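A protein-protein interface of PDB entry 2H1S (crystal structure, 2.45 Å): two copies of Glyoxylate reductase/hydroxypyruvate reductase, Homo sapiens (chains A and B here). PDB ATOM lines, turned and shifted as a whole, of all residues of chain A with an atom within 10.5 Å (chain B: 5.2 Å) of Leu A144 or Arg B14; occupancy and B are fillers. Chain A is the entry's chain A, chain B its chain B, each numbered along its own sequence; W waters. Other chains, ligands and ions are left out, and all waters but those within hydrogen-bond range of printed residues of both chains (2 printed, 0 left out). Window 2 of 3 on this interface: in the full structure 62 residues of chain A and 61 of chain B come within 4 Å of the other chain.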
ATOM      1  N   ARG A 125     -15.844  12.608   8.083  1.00  0.00           N
ATOM      2  CA  ARG A 125     -15.468  13.975   7.638  1.00  0.00           C
ATOM      3  C   ARG A 125     -14.328  14.633   8.439  1.00  0.00           C
ATOM      4  O   ARG A 125     -14.326  15.877   8.649  1.00  0.00           O
ATOM      5  CB  ARG A 125     -16.684  14.881   7.657  1.00  0.00           C
ATOM      6  CG  ARG A 125     -17.837  14.321   6.842  1.00  0.00           C
ATOM      7  CD  ARG A 125     -19.053  15.170   6.982  1.00  0.00           C
ATOM      8  NE  ARG A 125     -18.802  16.474   6.398  1.00  0.00           N
ATOM      9  CZ  ARG A 125     -19.664  17.477   6.396  1.00  0.00           C
ATOM     10  NH1 ARG A 125     -20.856  17.356   6.980  1.00  0.00           N
ATOM     11  NH2 ARG A 125     -19.320  18.617   5.827  1.00  0.00           N
ATOM     12  N   SER A 140     -17.861  26.574  18.723  1.00  0.00           N
ATOM     13  CA  SER A 140     -18.457  25.864  19.845  1.00  0.00           C
ATOM     14  C   SER A 140     -18.665  24.400  19.515  1.00  0.00           C
ATOM     15  O   SER A 140     -18.218  23.908  18.486  1.00  0.00           O
ATOM     16  CB  SER A 140     -19.803  26.454  20.199  1.00  0.00           C
ATOM     17  OG  SER A 140     -20.395  25.675  21.211  1.00  0.00           O
ATOM     18  N   TRP A 141     -19.357  23.684  20.394  1.00  0.00           N
ATOM     19  CA  TRP A 141     -19.946  22.423  19.969  1.00  0.00           C
ATOM     20  C   TRP A 141     -21.228  22.851  19.262  1.00  0.00           C
ATOM     21  O   TRP A 141     -21.897  23.767  19.720  1.00  0.00           O
ATOM     22  CB  TRP A 141     -20.200  21.543  21.159  1.00  0.00           C
ATOM     23  CG  TRP A 141     -20.727  20.177  20.866  1.00  0.00           C
ATOM     24  CD1 TRP A 141     -19.999  19.008  20.730  1.00  0.00           C
ATOM     25  CD2 TRP A 141     -22.105  19.811  20.739  1.00  0.00           C
ATOM     26  NE1 TRP A 141     -20.853  17.951  20.495  1.00  0.00           N
ATOM     27  CE2 TRP A 141     -22.148  18.421  20.511  1.00  0.00           C
ATOM     28  CE3 TRP A 141     -23.307  20.531  20.785  1.00  0.00           C
ATOM     29  CZ2 TRP A 141     -23.344  17.747  20.309  1.00  0.00           C
ATOM     30  CZ3 TRP A 141     -24.490  19.855  20.605  1.00  0.00           C
ATOM     31  CH2 TRP A 141     -24.505  18.478  20.373  1.00  0.00           C
ATOM     32  N   LYS A 142     -21.513  22.226  18.122  1.00  0.00           N
ATOM     33  CA  LYS A 142     -22.668  22.566  17.274  1.00  0.00           C
ATOM     34  C   LYS A 142     -23.428  21.296  16.900  1.00  0.00           C
ATOM     35  O   LYS A 142     -22.828  20.401  16.306  1.00  0.00           O
ATOM     36  CB  LYS A 142     -22.196  23.259  15.992  1.00  0.00           C
ATOM     37  CG  LYS A 142     -21.597  24.666  16.140  1.00  0.00           C
ATOM     38  CD  LYS A 142     -21.201  25.183  14.752  1.00  0.00           C
ATOM     39  CE  LYS A 142     -20.436  26.487  14.789  1.00  0.00           C
ATOM     40  NZ  LYS A 142     -21.155  27.682  14.302  1.00  0.00           N
ATOM     41  N   PRO A 143     -24.755  21.236  17.188  1.00  0.00           N
ATOM     42  CA  PRO A 143     -25.539  19.999  16.981  1.00  0.00           C
ATOM     43  C   PRO A 143     -25.693  19.598  15.497  1.00  0.00           C
ATOM     44  O   PRO A 143     -25.842  18.402  15.199  1.00  0.00           O
ATOM     45  CB  PRO A 143     -26.905  20.318  17.616  1.00  0.00           C
ATOM     46  CG  PRO A 143     -27.013  21.819  17.595  1.00  0.00           C
ATOM     47  CD  PRO A 143     -25.586  22.360  17.654  1.00  0.00           C
ATOM     48  N   LEU A 144     -25.637  20.585  14.596  1.00  0.00           N
ATOM     49  CA  LEU A 144     -25.942  20.391  13.170  1.00  0.00           C
ATOM     50  C   LEU A 144     -24.732  20.306  12.264  1.00  0.00           C
ATOM     51  O   LEU A 144     -24.869  20.266  11.048  1.00  0.00           O
ATOM     52  CB  LEU A 144     -26.753  21.582  12.684  1.00  0.00           C
ATOM     53  CG  LEU A 144     -28.129  21.668  13.293  1.00  0.00           C
ATOM     54  CD1 LEU A 144     -28.559  23.109  13.347  1.00  0.00           C
ATOM     55  CD2 LEU A 144     -29.093  20.791  12.456  1.00  0.00           C
ATOM     56  N   TRP A 145     -23.543  20.296  12.851  1.00  0.00           N
ATOM     57  CA  TRP A 145     -22.329  20.632  12.122  1.00  0.00           C
ATOM     58  C   TRP A 145     -21.418  19.444  11.994  1.00  0.00           C
ATOM     59  O   TRP A 145     -21.248  18.677  12.947  1.00  0.00           O
ATOM     60  CB  TRP A 145     -21.665  21.716  12.903  1.00  0.00           C
ATOM     61  CG  TRP A 145     -20.473  22.366  12.332  1.00  0.00           C
ATOM     62  CD1 TRP A 145     -20.398  23.124  11.187  1.00  0.00           C
ATOM     63  CD2 TRP A 145     -19.192  22.446  12.957  1.00  0.00           C
ATOM     64  NE1 TRP A 145     -19.127  23.627  11.052  1.00  0.00           N
ATOM     65  CE2 TRP A 145     -18.367  23.229  12.121  1.00  0.00           C
ATOM     66  CE3 TRP A 145     -18.662  21.941  14.151  1.00  0.00           C
ATOM     67  CZ2 TRP A 145     -17.027  23.505  12.435  1.00  0.00           C
ATOM     68  CZ3 TRP A 145     -17.306  22.197  14.454  1.00  0.00           C
ATOM     69  CH2 TRP A 145     -16.515  22.973  13.595  1.00  0.00           C
ATOM     70  N   LEU A 146     -20.853  19.285  10.793  1.00  0.00           N
ATOM     71  CA  LEU A 146     -19.930  18.201  10.456  1.00  0.00           C
ATOM     72  C   LEU A 146     -20.474  16.779  10.678  1.00  0.00           C
ATOM     73  O   LEU A 146     -19.698  15.828  10.982  1.00  0.00           O
ATOM     74  CB  LEU A 146     -18.582  18.407  11.146  1.00  0.00           C
ATOM     75  CG  LEU A 146     -17.479  19.171  10.414  1.00  0.00           C
ATOM     76  CD1 LEU A 146     -16.512  19.752  11.413  1.00  0.00           C
ATOM     77  CD2 LEU A 146     -16.746  18.220   9.554  1.00  0.00           C
ATOM     78  N   CYS A 147     -21.793  16.623  10.507  1.00  0.00           N
ATOM     79  CA  CYS A 147     -22.379  15.288  10.542  1.00  0.00           C
ATOM     80  C   CYS A 147     -22.139  14.554   9.253  1.00  0.00           C
ATOM     81  O   CYS A 147     -22.268  15.108   8.166  1.00  0.00           O
ATOM     82  CB  CYS A 147     -23.867  15.329  10.818  1.00  0.00           C
ATOM     83  SG  CYS A 147     -24.201  16.058  12.345  1.00  0.00           S
ATOM     84  N   GLY A 148     -21.739  13.303   9.400  1.00  0.00           N
ATOM     85  CA  GLY A 148     -21.596  12.384   8.300  1.00  0.00           C
ATOM     86  C   GLY A 148     -22.538  11.202   8.476  1.00  0.00           C
ATOM     87  O   GLY A 148     -23.544  11.269   9.216  1.00  0.00           O
ATOM     88  N   THR B  12     -31.339  26.899  23.989  1.00  0.00           N
ATOM     89  CA  THR B  12     -30.107  27.720  23.921  1.00  0.00           C
ATOM     90  C   THR B  12     -29.431  27.754  22.571  1.00  0.00           C
ATOM     91  O   THR B  12     -28.442  28.464  22.403  1.00  0.00           O
ATOM     92  CB  THR B  12     -29.009  27.324  24.959  1.00  0.00           C
ATOM     93  OG1 THR B  12     -28.490  26.033  24.642  1.00  0.00           O
ATOM     94  CG2 THR B  12     -29.578  27.303  26.394  1.00  0.00           C
ATOM     95  N   ARG B  13     -29.956  26.983  21.620  1.00  0.00           N
ATOM     96  CA  ARG B  13     -29.500  27.053  20.268  1.00  0.00           C
ATOM     97  C   ARG B  13     -30.497  26.515  19.250  1.00  0.00           C
ATOM     98  O   ARG B  13     -31.536  26.011  19.634  1.00  0.00           O
ATOM     99  CB  ARG B  13     -28.170  26.346  20.138  1.00  0.00           C
ATOM    100  CG  ARG B  13     -27.135  27.382  19.894  1.00  0.00           C
ATOM    101  CD  ARG B  13     -25.921  26.809  19.420  1.00  0.00           C
ATOM    102  NE  ARG B  13     -25.038  26.494  20.518  1.00  0.00           N
ATOM    103  CZ  ARG B  13     -23.813  26.032  20.326  1.00  0.00           C
ATOM    104  NH1 ARG B  13     -23.356  25.857  19.090  1.00  0.00           N
ATOM    105  NH2 ARG B  13     -23.071  25.731  21.364  1.00  0.00           N
ATOM    106  N   ARG B  14     -30.188  26.669  17.958  1.00  0.00           N
ATOM    107  CA  ARG B  14     -30.926  25.961  16.933  1.00  0.00           C
ATOM    108  C   ARG B  14     -30.557  24.504  17.067  1.00  0.00           C
ATOM    109  O   ARG B  14     -29.385  24.126  16.918  1.00  0.00           O
ATOM    110  CB  ARG B  14     -30.574  26.445  15.530  1.00  0.00           C
ATOM    111  CG  ARG B  14     -31.448  25.768  14.410  1.00  0.00           C
ATOM    112  CD  ARG B  14     -31.616  26.638  13.167  1.00  0.00           C
ATOM    113  NE  ARG B  14     -30.340  27.217  12.834  1.00  0.00           N
ATOM    114  CZ  ARG B  14     -30.103  28.496  12.604  1.00  0.00           C
ATOM    115  NH1 ARG B  14     -31.081  29.383  12.585  1.00  0.00           N
ATOM    116  NH2 ARG B  14     -28.855  28.877  12.366  1.00  0.00           N
ATOM    117  N   ILE B  15     -31.550  23.672  17.326  1.00  0.00           N
ATOM    118  CA  ILE B  15     -31.325  22.249  17.388  1.00  0.00           C
ATOM    119  C   ILE B  15     -31.863  21.513  16.143  1.00  0.00           C
ATOM    120  O   ILE B  15     -32.596  22.100  15.348  1.00  0.00           O
ATOM    121  CB  ILE B  15     -31.916  21.679  18.693  1.00  0.00           C
ATOM    122  CG1 ILE B  15     -33.453  21.792  18.701  1.00  0.00           C
ATOM    123  CG2 ILE B  15     -31.260  22.341  19.924  1.00  0.00           C
ATOM    124  CD1 ILE B  15     -34.121  20.982  19.827  1.00  0.00           C
ATOM    125  N   PRO B  16     -31.484  20.222  15.965  1.00  0.00           N
ATOM    126  CA  PRO B  16     -32.064  19.412  14.884  1.00  0.00           C
ATOM    127  C   PRO B  16     -33.584  19.468  14.843  1.00  0.00           C
ATOM    128  O   PRO B  16     -34.229  19.471  15.886  1.00  0.00           O
ATOM    129  CB  PRO B  16     -31.606  18.007  15.211  1.00  0.00           C
ATOM    130  CG  PRO B  16     -30.314  18.196  15.955  1.00  0.00           C
ATOM    131  CD  PRO B  16     -30.465  19.475  16.737  1.00  0.00           C
ATOM    132  N   ARG B  20     -37.042  20.282  17.597  1.00  0.00           N
ATOM    133  CA  ARG B  20     -37.784  21.563  17.576  1.00  0.00           C
ATOM    134  C   ARG B  20     -39.232  21.459  17.133  1.00  0.00           C
ATOM    135  O   ARG B  20     -40.065  22.222  17.606  1.00  0.00           O
ATOM    136  CB  ARG B  20     -37.091  22.714  16.815  1.00  0.00           C
ATOM    137  CG  ARG B  20     -36.025  22.363  15.829  1.00  0.00           C
ATOM    138  CD  ARG B  20     -35.386  23.643  15.221  1.00  0.00           C
ATOM    139  NE  ARG B  20     -34.863  23.358  13.883  1.00  0.00           N
ATOM    140  CZ  ARG B  20     -35.323  23.879  12.753  1.00  0.00           C
ATOM    141  NH1 ARG B  20     -36.307  24.769  12.762  1.00  0.00           N
ATOM    142  NH2 ARG B  20     -34.780  23.523  11.605  1.00  0.00           N
ATOM    143  N   GLN B  33     -36.383  30.583  21.682  1.00  0.00           N
ATOM    144  CA  GLN B  33     -35.202  29.977  21.132  1.00  0.00           C
ATOM    145  C   GLN B  33     -34.130  31.014  20.853  1.00  0.00           C
ATOM    146  O   GLN B  33     -34.423  32.108  20.363  1.00  0.00           O
ATOM    147  CB  GLN B  33     -35.564  29.262  19.821  1.00  0.00           C
ATOM    148  CG  GLN B  33     -34.471  28.361  19.298  1.00  0.00           C
ATOM    149  CD  GLN B  33     -35.024  27.157  18.534  1.00  0.00           C
ATOM    150  OE1 GLN B  33     -36.144  27.229  17.969  1.00  0.00           O
ATOM    151  NE2 GLN B  33     -34.253  26.030  18.524  1.00  0.00           N
ATOM    152  N   TRP B  34     -32.885  30.667  21.185  1.00  0.00           N
ATOM    153  CA  TRP B  34     -31.710  31.376  20.647  1.00  0.00           C
ATOM    154  C   TRP B  34     -31.577  30.916  19.183  1.00  0.00           C
ATOM    155  O   TRP B  34     -31.274  29.752  18.866  1.00  0.00           O
ATOM    156  CB  TRP B  34     -30.452  31.067  21.471  1.00  0.00           C
ATOM    157  CG  TRP B  34     -29.101  31.669  21.035  1.00  0.00           C
ATOM    158  CD1 TRP B  34     -28.001  30.969  20.595  1.00  0.00           C
ATOM    159  CD2 TRP B  34     -28.691  33.050  21.079  1.00  0.00           C
ATOM    160  NE1 TRP B  34     -26.954  31.827  20.332  1.00  0.00           N
ATOM    161  CE2 TRP B  34     -27.348  33.106  20.618  1.00  0.00           C
ATOM    162  CE3 TRP B  34     -29.321  34.240  21.455  1.00  0.00           C
ATOM    163  CZ2 TRP B  34     -26.632  34.305  20.528  1.00  0.00           C
ATOM    164  CZ3 TRP B  34     -28.601  35.449  21.358  1.00  0.00           C
ATOM    165  CH2 TRP B  34     -27.275  35.465  20.905  1.00  0.00           C
ATOM    166  N   ASP B  35     -31.828  31.878  18.314  1.00  0.00           N
ATOM    167  CA  ASP B  35     -32.049  31.704  16.894  1.00  0.00           C
ATOM    168  C   ASP B  35     -30.750  31.537  16.105  1.00  0.00           C
ATOM    169  O   ASP B  35     -30.603  32.140  15.029  1.00  0.00           O
ATOM    170  CB  ASP B  35     -32.698  33.022  16.474  1.00  0.00           C
ATOM    171  CG  ASP B  35     -32.152  34.248  17.331  1.00  0.00           C
ATOM    172  OD1 ASP B  35     -30.940  34.592  17.203  1.00  0.00           O
ATOM    173  OD2 ASP B  35     -32.916  34.842  18.145  1.00  0.00           O
ATOM    174  N   SER B  36     -29.799  30.751  16.611  1.00  0.00           N
ATOM    175  CA  SER B  36     -28.412  30.817  16.092  1.00  0.00           C
ATOM    176  C   SER B  36     -27.679  29.495  16.214  1.00  0.00           C
ATOM    177  O   SER B  36     -28.056  28.628  17.012  1.00  0.00           O
ATOM    178  CB  SER B  36     -27.623  31.935  16.820  1.00  0.00           C
ATOM    179  OG  SER B  36     -26.193  31.847  16.619  1.00  0.00           O
ATOM    180  N   ASP B  37     -26.652  29.339  15.389  1.00  0.00           N
ATOM    181  CA  ASP B  37     -25.708  28.222  15.483  1.00  0.00           C
ATOM    182  C   ASP B  37     -24.580  28.589  16.444  1.00  0.00           C
ATOM    183  O   ASP B  37     -23.910  27.730  16.970  1.00  0.00           O
ATOM    184  CB  ASP B  37     -25.097  27.920  14.120  1.00  0.00           C
ATOM    185  CG  ASP B  37     -26.082  27.240  13.149  1.00  0.00           C
ATOM    186  OD1 ASP B  37     -27.089  26.613  13.583  1.00  0.00           O
ATOM    187  OD2 ASP B  37     -25.815  27.320  11.925  1.00  0.00           O
ATOM    188  N   ARG B 302     -27.487  12.869  15.820  1.00  0.00           N
ATOM    189  CA  ARG B 302     -27.843  14.215  16.247  1.00  0.00           C
ATOM    190  C   ARG B 302     -29.338  14.422  16.304  1.00  0.00           C
ATOM    191  O   ARG B 302     -29.850  14.955  17.274  1.00  0.00           O
ATOM    192  CB  ARG B 302     -27.136  15.257  15.391  1.00  0.00           C
ATOM    193  CG  ARG B 302     -25.654  15.293  15.660  1.00  0.00           C
ATOM    194  CD  ARG B 302     -25.385  15.878  17.031  1.00  0.00           C
ATOM    195  NE  ARG B 302     -24.028  15.573  17.418  1.00  0.00           N
ATOM    196  CZ  ARG B 302     -22.979  16.309  17.072  1.00  0.00           C
ATOM    197  NH1 ARG B 302     -23.178  17.425  16.388  1.00  0.00           N
ATOM    198  NH2 ARG B 302     -21.749  15.924  17.420  1.00  0.00           N
HETATM  199  O   HOH W   1     -19.925  15.218  19.459  1.00  0.00           O
HETATM  200  O   HOH W   2     -20.376  18.653  15.579  1.00  0.00           O
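The side-chain hydroxyl (OG) of Ser A140 sits at hydrogen-bond distance from the guanidinium group (NH2) of Arg B13.
NH1 of Arg B13 lies within hydrogen-bond range of O of Trp A141, at 2.6 Å.
The guanidinium group (NH1) of Arg B302 lies within hydrogen-bond range of the backbone carbonyl oxygen (O) of Lys A142 (3.0 Å).
The backbone carbonyl oxygen of Pro A143 sits at hydrogen-bond distance from the guanidinium group of Arg B302.
O of Cys A147 lies within hydrogen-bond range of NH1 of Arg A125 (2.9 Å).
The side-chain amide nitrogen of Gln B33 lies within hydrogen-bond range of the backbone carbonyl oxygen of Arg B13, 2.9 Å away.
NH1 of Arg B13 sits at hydrogen-bond distance from O of Asp B37 (2.9 Å).
O of Trp B34 sits at hydrogen-bond distance from N of Arg B14, at 3.4 Å.
The backbone NH (N) of Arg B14 is in hydrogen-bond range of the backbone carbonyl oxygen (O) of Ser B36 (3.0 Å).
The guanidinium group (NH2) of Arg B14 is in salt-bridge range of the side-chain carboxylate (OD1) of Asp B37 (3.1 Å).
Among the printed residues, pairs that only touch across the chains: Trp A141 with Arg B302 (3.6 Å), Lys A142 with Arg B13 (3.6 Å), Lys A142 with Asp B37 (3.8 Å), Pro A143 with Arg B14 (3.4 Å), Pro A143 with Pro B16 (3.8 Å), Leu A144 with Arg B14 (3.8 Å), Leu A144 with Asp B37 (3.8 Å) and Cys A147 with Arg B302 (3.7 Å).
Printed residues of chain B within 4 Å of Pro A143: Arg B14, Pro B16 and Arg B302.
Of the printed residues of chain B, Leu A144 touches Arg B14 (3.8 Å) and Asp B37 (3.8 Å).
Of the printed residues of chain B, Cys A147 touches Arg B302.
Of the printed residues of chain A, Arg B14 touches Pro A143 (3.4 Å) and Leu A144 (3.8 Å).
Asp B37 touches two residues of chain A.
Of the 10 printed residues of chain A, 6 touch a printed residue of chain B.
Printed residues of chain A that touch a printed residue of chain B: Ser A140, Trp A141, Lys A142, Pro A143, Leu A144 and Cys A147.
Hydrophobic or aromatic side chains of chain A that line the printed part of chain B: Trp A141, Pro A143 and Leu A144.
Hydrophobic or aromatic side chains of chain B within 4 Å of the printed part of chain A: Pro B16.
Among the printed residues, no Asp or Glu carboxylate lies within 4 Å of a Lys or Arg side-chain nitrogen of the other chain.
No position is printed for both chains.
Of the 12 pairs that touch across the chains among the printed residues, none has its exchanged pair printed and touching as well.
Water W2 lies within hydrogen-bond range of the backbone carbonyl oxygen (O) of Trp A145 (2.8 Å), the backbone carbonyl oxygen (O) of Lys A142 (3.1 Å) and the guanidinium group (NH1) of Arg B302 (3.2 Å).
Water W1 lies within hydrogen-bond range of the guanidinium group of Arg B302 and the indole nitrogen of Trp A141.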
